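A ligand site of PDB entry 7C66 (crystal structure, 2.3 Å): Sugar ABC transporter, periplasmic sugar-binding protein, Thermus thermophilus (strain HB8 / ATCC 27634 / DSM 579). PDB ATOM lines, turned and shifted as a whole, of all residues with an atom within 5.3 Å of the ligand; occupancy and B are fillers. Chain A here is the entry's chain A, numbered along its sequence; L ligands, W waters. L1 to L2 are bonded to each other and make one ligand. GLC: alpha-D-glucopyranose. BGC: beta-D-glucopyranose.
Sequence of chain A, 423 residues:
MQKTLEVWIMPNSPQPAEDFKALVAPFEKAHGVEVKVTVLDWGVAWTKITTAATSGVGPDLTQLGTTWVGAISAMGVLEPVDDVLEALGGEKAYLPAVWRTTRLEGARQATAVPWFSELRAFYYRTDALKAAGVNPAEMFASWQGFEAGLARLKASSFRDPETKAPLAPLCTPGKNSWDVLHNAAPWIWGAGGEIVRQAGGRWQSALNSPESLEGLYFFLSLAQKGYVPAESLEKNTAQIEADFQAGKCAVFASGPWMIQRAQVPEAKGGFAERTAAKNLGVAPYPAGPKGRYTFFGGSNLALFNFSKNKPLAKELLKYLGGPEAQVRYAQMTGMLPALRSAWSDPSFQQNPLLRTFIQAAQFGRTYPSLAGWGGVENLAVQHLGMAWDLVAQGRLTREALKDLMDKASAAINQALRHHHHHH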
ATOM      1  N   ASN A  12     -17.686 -31.417   2.627  1.00  0.00           N
ATOM      2  CA  ASN A  12     -16.467 -32.259   2.703  1.00  0.00           C
ATOM      3  C   ASN A  12     -15.823 -32.454   1.313  1.00  0.00           C
ATOM      4  O   ASN A  12     -14.630 -32.807   1.264  1.00  0.00           O
ATOM      5  CB  ASN A  12     -16.811 -33.636   3.285  1.00  0.00           C
ATOM      6  CG  ASN A  12     -17.583 -33.548   4.587  1.00  0.00           C
ATOM      7  OD1 ASN A  12     -17.260 -32.722   5.434  1.00  0.00           O
ATOM      8  ND2 ASN A  12     -18.593 -34.382   4.747  1.00  0.00           N
ATOM      9  N   TRP A  42     -19.555 -24.874   7.201  1.00  0.00           N
ATOM     10  CA  TRP A  42     -18.905 -24.939   8.523  1.00  0.00           C
ATOM     11  C   TRP A  42     -19.244 -23.705   9.346  1.00  0.00           C
ATOM     12  O   TRP A  42     -19.392 -23.866  10.575  1.00  0.00           O
ATOM     13  CB  TRP A  42     -17.394 -25.154   8.394  1.00  0.00           C
ATOM     14  CG  TRP A  42     -17.030 -26.592   8.268  1.00  0.00           C
ATOM     15  CD1 TRP A  42     -16.570 -27.222   7.136  1.00  0.00           C
ATOM     16  CD2 TRP A  42     -17.138 -27.614   9.268  1.00  0.00           C
ATOM     17  NE1 TRP A  42     -16.356 -28.547   7.382  1.00  0.00           N
ATOM     18  CE2 TRP A  42     -16.686 -28.818   8.690  1.00  0.00           C
ATOM     19  CE3 TRP A  42     -17.599 -27.649  10.588  1.00  0.00           C
ATOM     20  CZ2 TRP A  42     -16.645 -30.011   9.403  1.00  0.00           C
ATOM     21  CZ3 TRP A  42     -17.541 -28.839  11.299  1.00  0.00           C
ATOM     22  CH2 TRP A  42     -17.095 -30.002  10.714  1.00  0.00           C
ATOM     23  N   GLN A  63     -23.479 -35.011  10.619  1.00  0.00           N
ATOM     24  CA  GLN A  63     -22.019 -34.891  10.753  1.00  0.00           C
ATOM     25  C   GLN A  63     -21.765 -34.025  11.979  1.00  0.00           C
ATOM     26  O   GLN A  63     -22.516 -33.096  12.154  1.00  0.00           O
ATOM     27  CB  GLN A  63     -21.403 -34.303   9.472  1.00  0.00           C
ATOM     28  CG  GLN A  63     -19.894 -34.283   9.487  1.00  0.00           C
ATOM     29  CD  GLN A  63     -19.381 -33.718   8.205  1.00  0.00           C
ATOM     30  OE1 GLN A  63     -20.109 -33.721   7.196  1.00  0.00           O
ATOM     31  NE2 GLN A  63     -18.137 -33.305   8.217  1.00  0.00           N
ATOM     32  N   GLY A  65     -18.073 -32.400  13.713  1.00  0.00           N
ATOM     33  CA  GLY A  65     -16.616 -32.292  13.866  1.00  0.00           C
ATOM     34  C   GLY A  65     -16.194 -33.018  15.137  1.00  0.00           C
ATOM     35  O   GLY A  65     -16.900 -32.973  16.089  1.00  0.00           O
ATOM     36  N   THR A  66     -15.101 -33.748  15.097  1.00  0.00           N
ATOM     37  CA  THR A  66     -14.574 -34.525  16.229  1.00  0.00           C
ATOM     38  C   THR A  66     -14.545 -33.633  17.475  1.00  0.00           C
ATOM     39  O   THR A  66     -14.883 -34.164  18.493  1.00  0.00           O
ATOM     40  CB  THR A  66     -13.225 -35.156  15.891  1.00  0.00           C
ATOM     41  OG1 THR A  66     -12.385 -34.084  15.455  1.00  0.00           O
ATOM     42  CG2 THR A  66     -13.370 -36.223  14.835  1.00  0.00           C
ATOM     43  N   THR A  67     -14.247 -32.348  17.374  1.00  0.00           N
ATOM     44  CA  THR A  67     -14.054 -31.457  18.551  1.00  0.00           C
ATOM     45  C   THR A  67     -15.404 -31.027  19.149  1.00  0.00           C
ATOM     46  O   THR A  67     -15.397 -30.485  20.319  1.00  0.00           O
ATOM     47  CB  THR A  67     -13.265 -30.163  18.223  1.00  0.00           C
ATOM     48  OG1 THR A  67     -14.054 -29.339  17.351  1.00  0.00           O
ATOM     49  CG2 THR A  67     -11.911 -30.464  17.609  1.00  0.00           C
ATOM     50  N   TRP A  68     -16.518 -31.319  18.457  1.00  0.00           N
ATOM     51  CA  TRP A  68     -17.884 -30.962  18.904  1.00  0.00           C
ATOM     52  C   TRP A  68     -18.594 -32.155  19.536  1.00  0.00           C
ATOM     53  O   TRP A  68     -19.739 -31.946  20.057  1.00  0.00           O
ATOM     54  CB  TRP A  68     -18.678 -30.426  17.747  1.00  0.00           C
ATOM     55  CG  TRP A  68     -18.185 -29.112  17.220  1.00  0.00           C
ATOM     56  CD1 TRP A  68     -17.166 -28.339  17.674  1.00  0.00           C
ATOM     57  CD2 TRP A  68     -18.689 -28.440  16.048  1.00  0.00           C
ATOM     58  NE1 TRP A  68     -17.044 -27.207  16.923  1.00  0.00           N
ATOM     59  CE2 TRP A  68     -17.956 -27.247  15.905  1.00  0.00           C
ATOM     60  CE3 TRP A  68     -19.730 -28.715  15.169  1.00  0.00           C
ATOM     61  CZ2 TRP A  68     -18.225 -26.343  14.894  1.00  0.00           C
ATOM     62  CZ3 TRP A  68     -19.993 -27.819  14.155  1.00  0.00           C
ATOM     63  CH2 TRP A  68     -19.231 -26.676  13.990  1.00  0.00           C
ATOM     64  N   PHE A 116     -14.537 -39.747   8.990  1.00  0.00           N
ATOM     65  CA  PHE A 116     -13.259 -39.469   8.305  1.00  0.00           C
ATOM     66  C   PHE A 116     -12.326 -38.712   9.250  1.00  0.00           C
ATOM     67  O   PHE A 116     -12.727 -38.146  10.298  1.00  0.00           O
ATOM     68  CB  PHE A 116     -13.512 -38.833   6.947  1.00  0.00           C
ATOM     69  CG  PHE A 116     -14.099 -37.441   7.005  1.00  0.00           C
ATOM     70  CD1 PHE A 116     -13.303 -36.351   7.309  1.00  0.00           C
ATOM     71  CD2 PHE A 116     -15.438 -37.226   6.723  1.00  0.00           C
ATOM     72  CE1 PHE A 116     -13.824 -35.071   7.333  1.00  0.00           C
ATOM     73  CE2 PHE A 116     -15.942 -35.936   6.703  1.00  0.00           C
ATOM     74  CZ  PHE A 116     -15.140 -34.869   7.035  1.00  0.00           C
ATOM     75  N   GLU A 118      -8.532 -36.311   9.313  1.00  0.00           N
ATOM     76  CA  GLU A 118      -8.097 -35.033   8.751  1.00  0.00           C
ATOM     77  C   GLU A 118      -6.961 -34.569   9.669  1.00  0.00           C
ATOM     78  O   GLU A 118      -7.188 -34.627  10.893  1.00  0.00           O
ATOM     79  CB  GLU A 118      -9.378 -34.218   8.909  1.00  0.00           C
ATOM     80  CG  GLU A 118      -9.401 -32.896   8.263  1.00  0.00           C
ATOM     81  CD  GLU A 118      -8.811 -31.802   9.113  1.00  0.00           C
ATOM     82  OE1 GLU A 118      -9.509 -31.151   9.863  1.00  0.00           O
ATOM     83  OE2 GLU A 118      -7.683 -31.550   8.842  1.00  0.00           O
ATOM     84  N   ARG A 120      -3.356 -31.597   9.637  1.00  0.00           N
ATOM     85  CA  ARG A 120      -2.801 -30.386   8.996  1.00  0.00           C
ATOM     86  C   ARG A 120      -1.310 -30.560   8.657  1.00  0.00           C
ATOM     87  O   ARG A 120      -0.550 -31.237   9.442  1.00  0.00           O
ATOM     88  CB  ARG A 120      -3.127 -29.194   9.900  1.00  0.00           C
ATOM     89  CG  ARG A 120      -4.614 -29.019  10.156  1.00  0.00           C
ATOM     90  CD  ARG A 120      -5.533 -28.935   8.932  1.00  0.00           C
ATOM     91  NE  ARG A 120      -6.929 -29.048   9.292  1.00  0.00           N
ATOM     92  CZ  ARG A 120      -7.692 -28.068   9.729  1.00  0.00           C
ATOM     93  NH1 ARG A 120      -7.215 -26.842   9.764  1.00  0.00           N
ATOM     94  NH2 ARG A 120      -8.947 -28.302  10.100  1.00  0.00           N
ATOM     95  N   SER A 177     -13.272 -18.521  10.843  1.00  0.00           N
ATOM     96  CA  SER A 177     -13.185 -19.977  10.607  1.00  0.00           C
ATOM     97  C   SER A 177     -12.831 -20.656  11.920  1.00  0.00           C
ATOM     98  O   SER A 177     -12.066 -20.073  12.684  1.00  0.00           O
ATOM     99  CB  SER A 177     -12.119 -20.271   9.575  1.00  0.00           C
ATOM    100  OG  SER A 177     -12.594 -19.873   8.300  1.00  0.00           O
ATOM    101  N   TRP A 178     -13.210 -21.918  12.055  1.00  0.00           N
ATOM    102  CA  TRP A 178     -12.711 -22.835  13.118  1.00  0.00           C
ATOM    103  C   TRP A 178     -11.185 -22.977  13.020  1.00  0.00           C
ATOM    104  O   TRP A 178     -10.535 -23.166  14.086  1.00  0.00           O
ATOM    105  CB  TRP A 178     -13.430 -24.191  13.057  1.00  0.00           C
ATOM    106  CG  TRP A 178     -14.917 -24.022  12.939  1.00  0.00           C
ATOM    107  CD1 TRP A 178     -15.705 -24.373  11.898  1.00  0.00           C
ATOM    108  CD2 TRP A 178     -15.770 -23.383  13.889  1.00  0.00           C
ATOM    109  NE1 TRP A 178     -17.009 -24.013  12.132  1.00  0.00           N
ATOM    110  CE2 TRP A 178     -17.080 -23.390  13.342  1.00  0.00           C
ATOM    111  CE3 TRP A 178     -15.561 -22.809  15.147  1.00  0.00           C
ATOM    112  CZ2 TRP A 178     -18.171 -22.845  13.997  1.00  0.00           C
ATOM    113  CZ3 TRP A 178     -16.660 -22.313  15.824  1.00  0.00           C
ATOM    114  CH2 TRP A 178     -17.938 -22.319  15.250  1.00  0.00           C
ATOM    115  N   ASP A 179     -10.639 -22.757  11.815  1.00  0.00           N
ATOM    116  CA  ASP A 179      -9.192 -22.913  11.534  1.00  0.00           C
ATOM    117  C   ASP A 179      -8.408 -21.737  12.143  1.00  0.00           C
ATOM    118  O   ASP A 179      -7.214 -21.855  12.276  1.00  0.00           O
ATOM    119  CB  ASP A 179      -8.926 -23.068  10.046  1.00  0.00           C
ATOM    120  CG  ASP A 179      -9.717 -24.229   9.452  1.00  0.00           C
ATOM    121  OD1 ASP A 179      -9.619 -25.365   9.980  1.00  0.00           O
ATOM    122  OD2 ASP A 179     -10.464 -23.980   8.490  1.00  0.00           O
ATOM    123  N   HIS A 182      -7.466 -23.860  14.871  1.00  0.00           N
ATOM    124  CA  HIS A 182      -6.684 -25.042  14.465  1.00  0.00           C
ATOM    125  C   HIS A 182      -5.293 -24.654  13.894  1.00  0.00           C
ATOM    126  O   HIS A 182      -4.340 -25.516  13.971  1.00  0.00           O
ATOM    127  CB  HIS A 182      -7.501 -25.885  13.503  1.00  0.00           C
ATOM    128  CG  HIS A 182      -8.825 -26.258  14.054  1.00  0.00           C
ATOM    129  ND1 HIS A 182      -9.026 -26.492  15.417  1.00  0.00           N
ATOM    130  CD2 HIS A 182     -10.042 -26.305  13.441  1.00  0.00           C
ATOM    131  CE1 HIS A 182     -10.320 -26.708  15.588  1.00  0.00           C
ATOM    132  NE2 HIS A 182     -10.977 -26.637  14.390  1.00  0.00           N
ATOM    133  N   THR A 237     -10.986 -19.278   5.771  1.00  0.00           N
ATOM    134  CA  THR A 237     -10.276 -20.458   5.225  1.00  0.00           C
ATOM    135  C   THR A 237     -10.608 -20.567   3.741  1.00  0.00           C
ATOM    136  O   THR A 237      -9.658 -20.746   2.934  1.00  0.00           O
ATOM    137  CB  THR A 237     -10.693 -21.749   5.909  1.00  0.00           C
ATOM    138  OG1 THR A 237      -9.998 -21.850   7.151  1.00  0.00           O
ATOM    139  CG2 THR A 237     -10.366 -22.979   5.082  1.00  0.00           C
ATOM    140  N   GLU A 241      -7.738 -20.633   0.824  1.00  0.00           N
ATOM    141  CA  GLU A 241      -7.686 -21.732  -0.174  1.00  0.00           C
ATOM    142  C   GLU A 241      -7.832 -21.136  -1.569  1.00  0.00           C
ATOM    143  O   GLU A 241      -7.072 -21.526  -2.462  1.00  0.00           O
ATOM    144  CB  GLU A 241      -8.813 -22.736  -0.012  1.00  0.00           C
ATOM    145  CG  GLU A 241      -8.458 -23.783   1.010  1.00  0.00           C
ATOM    146  CD  GLU A 241      -9.577 -24.723   1.413  1.00  0.00           C
ATOM    147  OE1 GLU A 241     -10.524 -24.862   0.615  1.00  0.00           O
ATOM    148  OE2 GLU A 241      -9.480 -25.286   2.532  1.00  0.00           O
ATOM    149  N   TRP A 257      -7.398 -32.773   1.758  1.00  0.00           N
ATOM    150  CA  TRP A 257      -8.437 -32.593   0.700  1.00  0.00           C
ATOM    151  C   TRP A 257      -7.856 -31.811  -0.477  1.00  0.00           C
ATOM    152  O   TRP A 257      -8.330 -32.040  -1.604  1.00  0.00           O
ATOM    153  CB  TRP A 257      -9.710 -31.915   1.240  1.00  0.00           C
ATOM    154  CG  TRP A 257      -9.488 -30.603   1.918  1.00  0.00           C
ATOM    155  CD1 TRP A 257      -9.365 -29.372   1.324  1.00  0.00           C
ATOM    156  CD2 TRP A 257      -9.335 -30.396   3.333  1.00  0.00           C
ATOM    157  NE1 TRP A 257      -9.173 -28.417   2.280  1.00  0.00           N
ATOM    158  CE2 TRP A 257      -9.065 -29.024   3.510  1.00  0.00           C
ATOM    159  CE3 TRP A 257      -9.363 -31.249   4.442  1.00  0.00           C
ATOM    160  CZ2 TRP A 257      -8.844 -28.485   4.769  1.00  0.00           C
ATOM    161  CZ3 TRP A 257      -9.090 -30.720   5.675  1.00  0.00           C
ATOM    162  CH2 TRP A 257      -8.854 -29.353   5.855  1.00  0.00           C
ATOM    163  N   PHE A 295      -2.487 -30.353  14.304  1.00  0.00           N
ATOM    164  CA  PHE A 295      -3.915 -30.551  14.569  1.00  0.00           C
ATOM    165  C   PHE A 295      -4.356 -31.806  13.830  1.00  0.00           C
ATOM    166  O   PHE A 295      -4.135 -31.933  12.585  1.00  0.00           O
ATOM    167  CB  PHE A 295      -4.719 -29.319  14.148  1.00  0.00           C
ATOM    168  CG  PHE A 295      -6.193 -29.578  14.269  1.00  0.00           C
ATOM    169  CD1 PHE A 295      -6.774 -29.645  15.512  1.00  0.00           C
ATOM    170  CD2 PHE A 295      -6.951 -29.864  13.156  1.00  0.00           C
ATOM    171  CE1 PHE A 295      -8.108 -29.982  15.645  1.00  0.00           C
ATOM    172  CE2 PHE A 295      -8.265 -30.247  13.301  1.00  0.00           C
ATOM    173  CZ  PHE A 295      -8.850 -30.296  14.527  1.00  0.00           C
ATOM    174  N   GLY A 297      -7.917 -34.024  13.517  1.00  0.00           N
ATOM    175  CA  GLY A 297      -9.366 -33.949  13.663  1.00  0.00           C
ATOM    176  C   GLY A 297     -10.048 -34.821  12.663  1.00  0.00           C
ATOM    177  O   GLY A 297      -9.625 -36.013  12.480  1.00  0.00           O
ATOM    178  N   GLY A 298     -11.121 -34.272  12.098  1.00  0.00           N
ATOM    179  CA  GLY A 298     -12.071 -34.956  11.212  1.00  0.00           C
ATOM    180  C   GLY A 298     -13.496 -34.810  11.705  1.00  0.00           C
ATOM    181  O   GLY A 298     -13.761 -33.883  12.491  1.00  0.00           O
ATOM    182  N   SER A 299     -14.350 -35.709  11.258  1.00  0.00           N
ATOM    183  CA  SER A 299     -15.799 -35.722  11.524  1.00  0.00           C
ATOM    184  C   SER A 299     -16.267 -37.144  11.782  1.00  0.00           C
ATOM    185  O   SER A 299     -15.785 -38.091  11.155  1.00  0.00           O
ATOM    186  CB  SER A 299     -16.556 -35.042  10.414  1.00  0.00           C
ATOM    187  OG  SER A 299     -16.335 -33.635  10.422  1.00  0.00           O
ATOM    188  N   MET A 335     -10.038 -36.983   2.117  1.00  0.00           N
ATOM    189  CA  MET A 335      -9.818 -37.196   3.562  1.00  0.00           C
ATOM    190  C   MET A 335      -9.208 -38.585   3.751  1.00  0.00           C
ATOM    191  O   MET A 335      -9.173 -39.368   2.793  1.00  0.00           O
ATOM    192  CB  MET A 335     -11.115 -37.085   4.373  1.00  0.00           C
ATOM    193  CG  MET A 335     -11.852 -35.797   4.174  1.00  0.00           C
ATOM    194  SD  MET A 335     -11.074 -34.320   4.846  1.00  0.00           S
ATOM    195  CE  MET A 335     -12.310 -33.141   4.294  1.00  0.00           C
ATOM    196  N   GLU A 377     -14.586 -22.891  21.129  1.00  0.00           N
ATOM    197  CA  GLU A 377     -14.109 -22.638  19.756  1.00  0.00           C
ATOM    198  C   GLU A 377     -14.613 -21.281  19.274  1.00  0.00           C
ATOM    199  O   GLU A 377     -13.768 -20.548  18.762  1.00  0.00           O
ATOM    200  CB  GLU A 377     -14.469 -23.796  18.827  1.00  0.00           C
ATOM    201  CG  GLU A 377     -13.624 -25.031  19.067  1.00  0.00           C
ATOM    202  CD  GLU A 377     -13.544 -26.039  17.938  1.00  0.00           C
ATOM    203  OE1 GLU A 377     -14.336 -25.934  16.977  1.00  0.00           O
ATOM    204  OE2 GLU A 377     -12.735 -26.964  18.075  1.00  0.00           O
HETATM  205  C1  GLC L   1     -13.129 -26.883   6.750  1.00  0.00           C
HETATM  206  C2  GLC L   1     -13.276 -26.123   8.103  1.00  0.00           C
HETATM  207  C3  GLC L   1     -12.705 -26.810   9.344  1.00  0.00           C
HETATM  208  C4  GLC L   1     -12.829 -28.307   9.229  1.00  0.00           C
HETATM  209  C5  GLC L   1     -12.194 -28.792   7.934  1.00  0.00           C
HETATM  210  C6  GLC L   1     -12.319 -30.296   7.741  1.00  0.00           C
HETATM  211  O1  GLC L   1     -12.209 -26.216   5.953  1.00  0.00           O
HETATM  212  O2  GLC L   1     -12.810 -24.758   7.984  1.00  0.00           O
HETATM  213  O3  GLC L   1     -13.471 -26.406  10.493  1.00  0.00           O
HETATM  214  O4  GLC L   1     -12.143 -28.870  10.323  1.00  0.00           O
HETATM  215  O5  GLC L   1     -12.708 -28.235   6.737  1.00  0.00           O
HETATM  216  O6  GLC L   1     -13.663 -30.667   7.599  1.00  0.00           O
HETATM  217  C2  BGC L   2     -12.127 -30.540  12.044  1.00  0.00           C
HETATM  218  C3  BGC L   2     -12.912 -31.042  13.267  1.00  0.00           C
HETATM  219  C4  BGC L   2     -13.533 -29.921  14.105  1.00  0.00           C
HETATM  220  C5  BGC L   2     -14.227 -28.911  13.217  1.00  0.00           C
HETATM  221  C6  BGC L   2     -14.717 -27.688  13.982  1.00  0.00           C
HETATM  222  C1  BGC L   2     -12.924 -29.484  11.309  1.00  0.00           C
HETATM  223  O2  BGC L   2     -11.946 -31.619  11.133  1.00  0.00           O
HETATM  224  O3  BGC L   2     -12.058 -31.865  14.085  1.00  0.00           O
HETATM  225  O4  BGC L   2     -14.406 -30.462  15.092  1.00  0.00           O
HETATM  226  O5  BGC L   2     -13.291 -28.459  12.205  1.00  0.00           O
HETATM  227  O6  BGC L   2     -13.654 -27.092  14.760  1.00  0.00           O
HETATM  228  O   HOH W   1     -13.896 -32.632   9.524  1.00  0.00           O
HETATM  229  O   HOH W   2     -14.465 -22.708   9.342  1.00  0.00           O
HETATM  230  O   HOH W   3     -12.750 -28.717   3.571  1.00  0.00           O
HETATM  231  O   HOH W   4     -11.819 -26.492   3.380  1.00  0.00           O
HETATM  232  O   HOH W   5     -15.300 -30.709   5.663  1.00  0.00           O
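OD2 of Asp 179 is in hydrogen-bond range of O2 of GLC L1 (2.5 Å).
The backbone NH of Thr 67 lies within hydrogen-bond range of an oxygen (O4) of BGC L2 (3.0 Å).
An oxygen (O4) of BGC L2 is in hydrogen-bond range of the side-chain hydroxyl (OG1) of Thr 67 (2.5 Å).
OE1 of Glu 377 sits at hydrogen-bond distance from O6 of BGC L2.
N of Thr 66 is in hydrogen-bond range of O4 of BGC L2, 3.4 Å away.
The side-chain hydroxyl (OG1) of Thr 66 lies within hydrogen-bond range of an oxygen (O3) of BGC L2 (2.6 Å).
An oxygen (O6) of BGC L2 sits at hydrogen-bond distance from a ring nitrogen (NE2) of His 182, 2.7 Å away.
OE1 of Glu 118 sits at hydrogen-bond distance from O2 of BGC L2, at 2.8 Å.
The backbone NH (N) of Gly 298 is in hydrogen-bond range of an oxygen (O2) of BGC L2 (2.9 Å).
The backbone carbonyl oxygen (O) of Gly 298 sits close to an oxygen (O3) of BGC L2, at 3.1 Å.
NH2 of Arg 120 is in hydrogen-bond range of O4 of GLC L1, at 3.3 Å.
The indole nitrogen of Trp 42 lies within hydrogen-bond range of an oxygen (O6) of GLC L1 (3.4 Å).
The side-chain carboxylate of Asp 179 is in salt-bridge range of the guanidinium group of Arg 120, at 2.8 Å.
The side-chain carboxylate of Asp 179 lies within hydrogen-bond range of the side-chain hydroxyl of Thr 237, 2.6 Å away.
The indole nitrogen (NE1) of Trp 68 sits at hydrogen-bond distance from the side-chain carboxylate (OE1) of Glu 377 (3.0 Å).
O of Gly 298 sits at hydrogen-bond distance from N of Thr 66 (2.9 Å).
The side-chain carboxylate (OE2) of Glu 118 is in salt-bridge range of the guanidinium group (NE) of Arg 120, 2.7 Å away.
The backbone carbonyl oxygen (O) of Glu 118 is in hydrogen-bond range of the backbone NH (N) of Gly 297 (2.8 Å).
The backbone NH (N) of Arg 120 sits at hydrogen-bond distance from the backbone carbonyl oxygen (O) of Phe 295 (3.1 Å).
OE2 of Glu 241 lies within hydrogen-bond range of NE1 of Trp 257.
C of Gly 65 touches O4 of BGC L2, 3.1 Å away.
NE1 of Trp 68 touches C6 of BGC L2 (3.8 Å).
CD1 of Trp 178 touches O3 of GLC L1, at 3.3 Å.
CG2 of Thr 237 touches O1 of GLC L1, 3.8 Å away.
CZ3 of Trp 257 touches C6 of GLC L1, 3.9 Å away.
CZ of Phe 295 touches O3 of BGC L2 (3.6 Å).
CA of Gly 297 touches O3 of BGC L2 (3.4 Å).
16 residues have an atom within 4 Å of the ligand: Trp 42, Gly 65, Thr 66, Thr 67, Trp 68, Glu 118, Arg 120, Trp 178, Asp 179, His 182, Thr 237, Trp 257, Phe 295, Gly 297, Gly 298 and Glu 377.
Water W5 lies within hydrogen-bond range of an oxygen (O6) of GLC L1, the side-chain amide oxygen (OD1) of Asn 12 and the indole nitrogen (NE1) of Trp 42.
Water W4 lies within hydrogen-bond range of O1 of GLC L1, OE2 of Glu 241 and NE1 of Trp 257.
Water W1 lies within hydrogen-bond range of an oxygen (O2) of BGC L2 (2.7 Å), the side-chain hydroxyl of Ser 299 (2.8 Å) and the backbone carbonyl oxygen of Gly 298 (3.2 Å).
Water W2 lies within hydrogen-bond range of an oxygen (O2) of GLC L1 (3.0 Å) and the backbone NH of Trp 178 (3.1 Å).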
